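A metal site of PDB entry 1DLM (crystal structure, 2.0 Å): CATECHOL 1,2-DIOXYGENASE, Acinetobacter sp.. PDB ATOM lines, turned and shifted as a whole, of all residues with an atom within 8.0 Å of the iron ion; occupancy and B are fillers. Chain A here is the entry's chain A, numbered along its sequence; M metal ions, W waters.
N of His 226 lies within hydrogen-bond range of O of Trp 156 (3.0 Å).
A ring nitrogen (ND1) of His 226 is in hydrogen-bond range of the backbone carbonyl oxygen (O) of Glu 106.
A ring nitrogen (ND1) of His 224 lies within hydrogen-bond range of the backbone carbonyl oxygen (O) of Pro 222, at 2.8 Å.
O of Tyr 200 sits at hydrogen-bond distance from N of Arg 221 (2.8 Å).
NH1 of Arg 221 touches the iron ion, 3.9 Å away.
Five residues have an atom within 4 Å of the iron ion: Tyr 164, Tyr 200, Arg 221, His 224 and His 226.
The nearest printed residue that does not touch the iron ion is Leu 109 (4.8 Å).
The iron ion is bound by the side-chain hydroxyl of Tyr 164 (1.8 Å), a ring nitrogen (NE2) of His 226 (2.0 Å), a ring nitrogen (NE2) of His 224 (2.2 Å), the side-chain hydroxyl of Tyr 200 (2.3 Å) and water W1 (2.4 Å).
The iron ion has five donor atoms within binding distance.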
ATOM      1  N   ILE A 105     -14.761   7.407 -25.424  1.00  0.00           N
ATOM      2  CA  ILE A 105     -13.801   8.472 -25.171  1.00  0.00           C
ATOM      3  C   ILE A 105     -14.302   9.687 -24.409  1.00  0.00           C
ATOM      4  O   ILE A 105     -15.455  10.092 -24.511  1.00  0.00           O
ATOM      5  CB  ILE A 105     -13.098   8.926 -26.457  1.00  0.00           C
ATOM      6  CG1 ILE A 105     -14.012   9.824 -27.282  1.00  0.00           C
ATOM      7  CG2 ILE A 105     -12.694   7.703 -27.245  1.00  0.00           C
ATOM      8  CD1 ILE A 105     -13.336  10.403 -28.507  1.00  0.00           C
ATOM      9  N   GLU A 106     -13.405  10.250 -23.622  1.00  0.00           N
ATOM     10  CA  GLU A 106     -13.698  11.411 -22.817  1.00  0.00           C
ATOM     11  C   GLU A 106     -13.709  12.689 -23.633  1.00  0.00           C
ATOM     12  O   GLU A 106     -14.538  13.555 -23.402  1.00  0.00           O
ATOM     13  CB  GLU A 106     -12.656  11.528 -21.702  1.00  0.00           C
ATOM     14  CG  GLU A 106     -12.652  12.850 -20.973  1.00  0.00           C
ATOM     15  CD  GLU A 106     -11.526  12.933 -19.976  1.00  0.00           C
ATOM     16  OE1 GLU A 106     -10.983  11.862 -19.589  1.00  0.00           O
ATOM     17  OE2 GLU A 106     -11.185  14.058 -19.564  1.00  0.00           O
ATOM     18  N   GLY A 107     -12.809  12.798 -24.609  1.00  0.00           N
ATOM     19  CA  GLY A 107     -12.738  14.014 -25.393  1.00  0.00           C
ATOM     20  C   GLY A 107     -11.795  14.989 -24.686  1.00  0.00           C
ATOM     21  O   GLY A 107     -11.424  14.773 -23.531  1.00  0.00           O
ATOM     22  N   PRO A 108     -11.374  16.065 -25.357  1.00  0.00           N
ATOM     23  CA  PRO A 108     -10.452  17.039 -24.761  1.00  0.00           C
ATOM     24  C   PRO A 108     -11.107  18.254 -24.090  1.00  0.00           C
ATOM     25  O   PRO A 108     -10.418  19.205 -23.713  1.00  0.00           O
ATOM     26  CB  PRO A 108      -9.630  17.444 -25.972  1.00  0.00           C
ATOM     27  CG  PRO A 108     -10.752  17.652 -26.976  1.00  0.00           C
ATOM     28  CD  PRO A 108     -11.634  16.419 -26.763  1.00  0.00           C
ATOM     29  N   LEU A 109     -12.427  18.225 -23.915  1.00  0.00           N
ATOM     30  CA  LEU A 109     -13.107  19.384 -23.374  1.00  0.00           C
ATOM     31  C   LEU A 109     -13.668  19.350 -21.957  1.00  0.00           C
ATOM     32  O   LEU A 109     -14.521  20.160 -21.628  1.00  0.00           O
ATOM     33  CB  LEU A 109     -14.221  19.786 -24.347  1.00  0.00           C
ATOM     34  CG  LEU A 109     -13.683  19.948 -25.776  1.00  0.00           C
ATOM     35  CD1 LEU A 109     -14.833  20.184 -26.731  1.00  0.00           C
ATOM     36  CD2 LEU A 109     -12.670  21.090 -25.815  1.00  0.00           C
ATOM     37  N   TYR A 110     -13.202  18.431 -21.125  1.00  0.00           N
ATOM     38  CA  TYR A 110     -13.679  18.381 -19.748  1.00  0.00           C
ATOM     39  C   TYR A 110     -13.075  19.542 -18.948  1.00  0.00           C
ATOM     40  O   TYR A 110     -11.953  19.959 -19.215  1.00  0.00           O
ATOM     41  CB  TYR A 110     -13.246  17.074 -19.080  1.00  0.00           C
ATOM     42  CG  TYR A 110     -13.550  17.012 -17.601  1.00  0.00           C
ATOM     43  CD1 TYR A 110     -14.850  16.815 -17.137  1.00  0.00           C
ATOM     44  CD2 TYR A 110     -12.530  17.147 -16.651  1.00  0.00           C
ATOM     45  CE1 TYR A 110     -15.122  16.762 -15.768  1.00  0.00           C
ATOM     46  CE2 TYR A 110     -12.792  17.092 -15.283  1.00  0.00           C
ATOM     47  CZ  TYR A 110     -14.096  16.897 -14.860  1.00  0.00           C
ATOM     48  OH  TYR A 110     -14.341  16.833 -13.514  1.00  0.00           O
ATOM     49  N   TRP A 156     -21.334  17.252 -19.252  1.00  0.00           N
ATOM     50  CA  TRP A 156     -20.947  18.434 -19.992  1.00  0.00           C
ATOM     51  C   TRP A 156     -21.293  18.217 -21.454  1.00  0.00           C
ATOM     52  O   TRP A 156     -21.283  17.083 -21.946  1.00  0.00           O
ATOM     53  CB  TRP A 156     -19.449  18.766 -19.791  1.00  0.00           C
ATOM     54  CG  TRP A 156     -18.394  17.796 -20.311  1.00  0.00           C
ATOM     55  CD1 TRP A 156     -17.585  17.965 -21.420  1.00  0.00           C
ATOM     56  CD2 TRP A 156     -17.982  16.560 -19.716  1.00  0.00           C
ATOM     57  NE1 TRP A 156     -16.706  16.908 -21.527  1.00  0.00           N
ATOM     58  CE2 TRP A 156     -16.923  16.030 -20.503  1.00  0.00           C
ATOM     59  CE3 TRP A 156     -18.401  15.834 -18.580  1.00  0.00           C
ATOM     60  CZ2 TRP A 156     -16.285  14.827 -20.194  1.00  0.00           C
ATOM     61  CZ3 TRP A 156     -17.763  14.631 -18.272  1.00  0.00           C
ATOM     62  CH2 TRP A 156     -16.718  14.139 -19.085  1.00  0.00           C
ATOM     63  N   HIS A 157     -21.655  19.298 -22.128  1.00  0.00           N
ATOM     64  CA  HIS A 157     -22.025  19.216 -23.521  1.00  0.00           C
ATOM     65  C   HIS A 157     -22.051  20.609 -24.132  1.00  0.00           C
ATOM     66  O   HIS A 157     -21.897  21.603 -23.419  1.00  0.00           O
ATOM     67  CB  HIS A 157     -23.391  18.543 -23.672  1.00  0.00           C
ATOM     68  CG  HIS A 157     -24.531  19.359 -23.129  1.00  0.00           C
ATOM     69  ND1 HIS A 157     -25.029  20.464 -23.777  1.00  0.00           N
ATOM     70  CD2 HIS A 157     -25.241  19.241 -21.982  1.00  0.00           C
ATOM     71  CE1 HIS A 157     -26.004  20.991 -23.064  1.00  0.00           C
ATOM     72  NE2 HIS A 157     -26.147  20.271 -21.969  1.00  0.00           N
ATOM     73  N   ALA A 158     -22.245  20.669 -25.435  1.00  0.00           N
ATOM     74  CA  ALA A 158     -22.252  21.926 -26.164  1.00  0.00           C
ATOM     75  C   ALA A 158     -23.642  22.528 -26.304  1.00  0.00           C
ATOM     76  O   ALA A 158     -24.643  21.885 -25.957  1.00  0.00           O
ATOM     77  CB  ALA A 158     -21.640  21.723 -27.561  1.00  0.00           C
ATOM     78  N   GLY A 162     -22.707  24.364 -31.152  1.00  0.00           N
ATOM     79  CA  GLY A 162     -21.641  23.389 -31.013  1.00  0.00           C
ATOM     80  C   GLY A 162     -20.452  23.795 -30.144  1.00  0.00           C
ATOM     81  O   GLY A 162     -19.375  23.198 -30.259  1.00  0.00           O
ATOM     82  N   TYR A 164     -18.687  24.552 -26.275  1.00  0.00           N
ATOM     83  CA  TYR A 164     -18.737  24.235 -24.853  1.00  0.00           C
ATOM     84  C   TYR A 164     -18.227  25.464 -24.115  1.00  0.00           C
ATOM     85  O   TYR A 164     -17.422  26.229 -24.655  1.00  0.00           O
ATOM     86  CB  TYR A 164     -17.801  23.088 -24.485  1.00  0.00           C
ATOM     87  CG  TYR A 164     -18.137  21.730 -25.036  1.00  0.00           C
ATOM     88  CD1 TYR A 164     -18.037  21.442 -26.404  1.00  0.00           C
ATOM     89  CD2 TYR A 164     -18.488  20.697 -24.167  1.00  0.00           C
ATOM     90  CE1 TYR A 164     -18.275  20.164 -26.882  1.00  0.00           C
ATOM     91  CE2 TYR A 164     -18.727  19.411 -24.633  1.00  0.00           C
ATOM     92  CZ  TYR A 164     -18.619  19.154 -25.998  1.00  0.00           C
ATOM     93  OH  TYR A 164     -18.882  17.888 -26.444  1.00  0.00           O
ATOM     94  N   ALA A 198     -25.812  20.438 -30.008  1.00  0.00           N
ATOM     95  CA  ALA A 198     -25.730  20.282 -31.452  1.00  0.00           C
ATOM     96  C   ALA A 198     -24.369  19.650 -31.642  1.00  0.00           C
ATOM     97  O   ALA A 198     -23.475  19.874 -30.827  1.00  0.00           O
ATOM     98  CB  ALA A 198     -25.781  21.642 -32.134  1.00  0.00           C
ATOM     99  N   TYR A 200     -20.686  19.105 -33.513  1.00  0.00           N
ATOM    100  CA  TYR A 200     -19.713  20.147 -33.835  1.00  0.00           C
ATOM    101  C   TYR A 200     -18.554  19.556 -34.613  1.00  0.00           C
ATOM    102  O   TYR A 200     -18.325  18.344 -34.573  1.00  0.00           O
ATOM    103  CB  TYR A 200     -19.206  20.832 -32.563  1.00  0.00           C
ATOM    104  CG  TYR A 200     -18.577  19.884 -31.574  1.00  0.00           C
ATOM    105  CD1 TYR A 200     -17.231  19.505 -31.680  1.00  0.00           C
ATOM    106  CD2 TYR A 200     -19.336  19.331 -30.538  1.00  0.00           C
ATOM    107  CE1 TYR A 200     -16.663  18.601 -30.783  1.00  0.00           C
ATOM    108  CE2 TYR A 200     -18.787  18.431 -29.639  1.00  0.00           C
ATOM    109  CZ  TYR A 200     -17.452  18.060 -29.766  1.00  0.00           C
ATOM    110  OH  TYR A 200     -16.918  17.142 -28.872  1.00  0.00           O
ATOM    111  N   ARG A 221     -18.649  15.675 -35.384  1.00  0.00           N
ATOM    112  CA  ARG A 221     -19.106  14.778 -34.342  1.00  0.00           C
ATOM    113  C   ARG A 221     -20.624  14.935 -34.218  1.00  0.00           C
ATOM    114  O   ARG A 221     -21.152  16.046 -34.327  1.00  0.00           O
ATOM    115  CB  ARG A 221     -18.495  15.115 -32.984  1.00  0.00           C
ATOM    116  CG  ARG A 221     -16.978  15.145 -32.939  1.00  0.00           C
ATOM    117  CD  ARG A 221     -16.524  14.825 -31.528  1.00  0.00           C
ATOM    118  NE  ARG A 221     -16.883  13.453 -31.217  1.00  0.00           N
ATOM    119  CZ  ARG A 221     -16.763  12.891 -30.017  1.00  0.00           C
ATOM    120  NH1 ARG A 221     -16.294  13.599 -28.992  1.00  0.00           N
ATOM    121  NH2 ARG A 221     -17.123  11.622 -29.850  1.00  0.00           N
ATOM    122  N   PRO A 222     -21.346  13.829 -34.033  1.00  0.00           N
ATOM    123  CA  PRO A 222     -22.806  13.925 -33.894  1.00  0.00           C
ATOM    124  C   PRO A 222     -23.103  14.568 -32.529  1.00  0.00           C
ATOM    125  O   PRO A 222     -22.222  14.627 -31.668  1.00  0.00           O
ATOM    126  CB  PRO A 222     -23.242  12.468 -33.967  1.00  0.00           C
ATOM    127  CG  PRO A 222     -22.079  11.763 -33.259  1.00  0.00           C
ATOM    128  CD  PRO A 222     -20.929  12.409 -33.999  1.00  0.00           C
ATOM    129  N   ALA A 223     -24.333  15.049 -32.327  1.00  0.00           N
ATOM    130  CA  ALA A 223     -24.677  15.660 -31.052  1.00  0.00           C
ATOM    131  C   ALA A 223     -24.535  14.610 -29.951  1.00  0.00           C
ATOM    132  O   ALA A 223     -24.951  13.460 -30.131  1.00  0.00           O
ATOM    133  CB  ALA A 223     -26.091  16.199 -31.082  1.00  0.00           C
ATOM    134  N   HIS A 224     -23.918  14.983 -28.838  1.00  0.00           N
ATOM    135  CA  HIS A 224     -23.711  14.042 -27.748  1.00  0.00           C
ATOM    136  C   HIS A 224     -23.566  14.726 -26.394  1.00  0.00           C
ATOM    137  O   HIS A 224     -23.349  15.947 -26.313  1.00  0.00           O
ATOM    138  CB  HIS A 224     -22.461  13.212 -27.985  1.00  0.00           C
ATOM    139  CG  HIS A 224     -21.222  14.035 -28.115  1.00  0.00           C
ATOM    140  ND1 HIS A 224     -20.925  14.767 -29.245  1.00  0.00           N
ATOM    141  CD2 HIS A 224     -20.261  14.339 -27.212  1.00  0.00           C
ATOM    142  CE1 HIS A 224     -19.834  15.478 -29.041  1.00  0.00           C
ATOM    143  NE2 HIS A 224     -19.411  15.236 -27.816  1.00  0.00           N
ATOM    144  N   ILE A 225     -23.641  13.919 -25.342  1.00  0.00           N
ATOM    145  CA  ILE A 225     -23.537  14.424 -23.986  1.00  0.00           C
ATOM    146  C   ILE A 225     -22.543  13.553 -23.240  1.00  0.00           C
ATOM    147  O   ILE A 225     -22.647  12.334 -23.214  1.00  0.00           O
ATOM    148  CB  ILE A 225     -24.922  14.384 -23.284  1.00  0.00           C
ATOM    149  CG1 ILE A 225     -25.944  15.176 -24.124  1.00  0.00           C
ATOM    150  CG2 ILE A 225     -24.807  14.963 -21.873  1.00  0.00           C
ATOM    151  CD1 ILE A 225     -27.367  15.126 -23.589  1.00  0.00           C
ATOM    152  N   HIS A 226     -21.558  14.221 -22.642  1.00  0.00           N
ATOM    153  CA  HIS A 226     -20.486  13.559 -21.919  1.00  0.00           C
ATOM    154  C   HIS A 226     -20.837  13.225 -20.481  1.00  0.00           C
ATOM    155  O   HIS A 226     -21.508  14.006 -19.802  1.00  0.00           O
ATOM    156  CB  HIS A 226     -19.246  14.464 -21.921  1.00  0.00           C
ATOM    157  CG  HIS A 226     -18.678  14.729 -23.283  1.00  0.00           C
ATOM    158  ND1 HIS A 226     -17.805  13.857 -23.901  1.00  0.00           N
ATOM    159  CD2 HIS A 226     -18.854  15.750 -24.136  1.00  0.00           C
ATOM    160  CE1 HIS A 226     -17.478  14.340 -25.087  1.00  0.00           C
ATOM    161  NE2 HIS A 226     -18.104  15.490 -25.252  1.00  0.00           N
ATOM    162  N   GLN A 240     -20.668   8.432 -22.857  1.00  0.00           N
ATOM    163  CA  GLN A 240     -21.472   9.509 -23.404  1.00  0.00           C
ATOM    164  C   GLN A 240     -22.710   8.925 -24.045  1.00  0.00           C
ATOM    165  O   GLN A 240     -22.853   7.696 -24.186  1.00  0.00           O
ATOM    166  CB  GLN A 240     -20.674  10.280 -24.459  1.00  0.00           C
ATOM    167  CG  GLN A 240     -20.657   9.582 -25.814  1.00  0.00           C
ATOM    168  CD  GLN A 240     -19.966  10.391 -26.892  1.00  0.00           C
ATOM    169  OE1 GLN A 240     -20.117  10.103 -28.080  1.00  0.00           O
ATOM    170  NE2 GLN A 240     -19.202  11.393 -26.496  1.00  0.00           N
HETATM  171 FE    FE M   1     -17.893  16.516 -26.904  1.00  0.00          FE
HETATM  172  O   HOH W   1     -15.488  16.595 -26.843  1.00  0.00           O
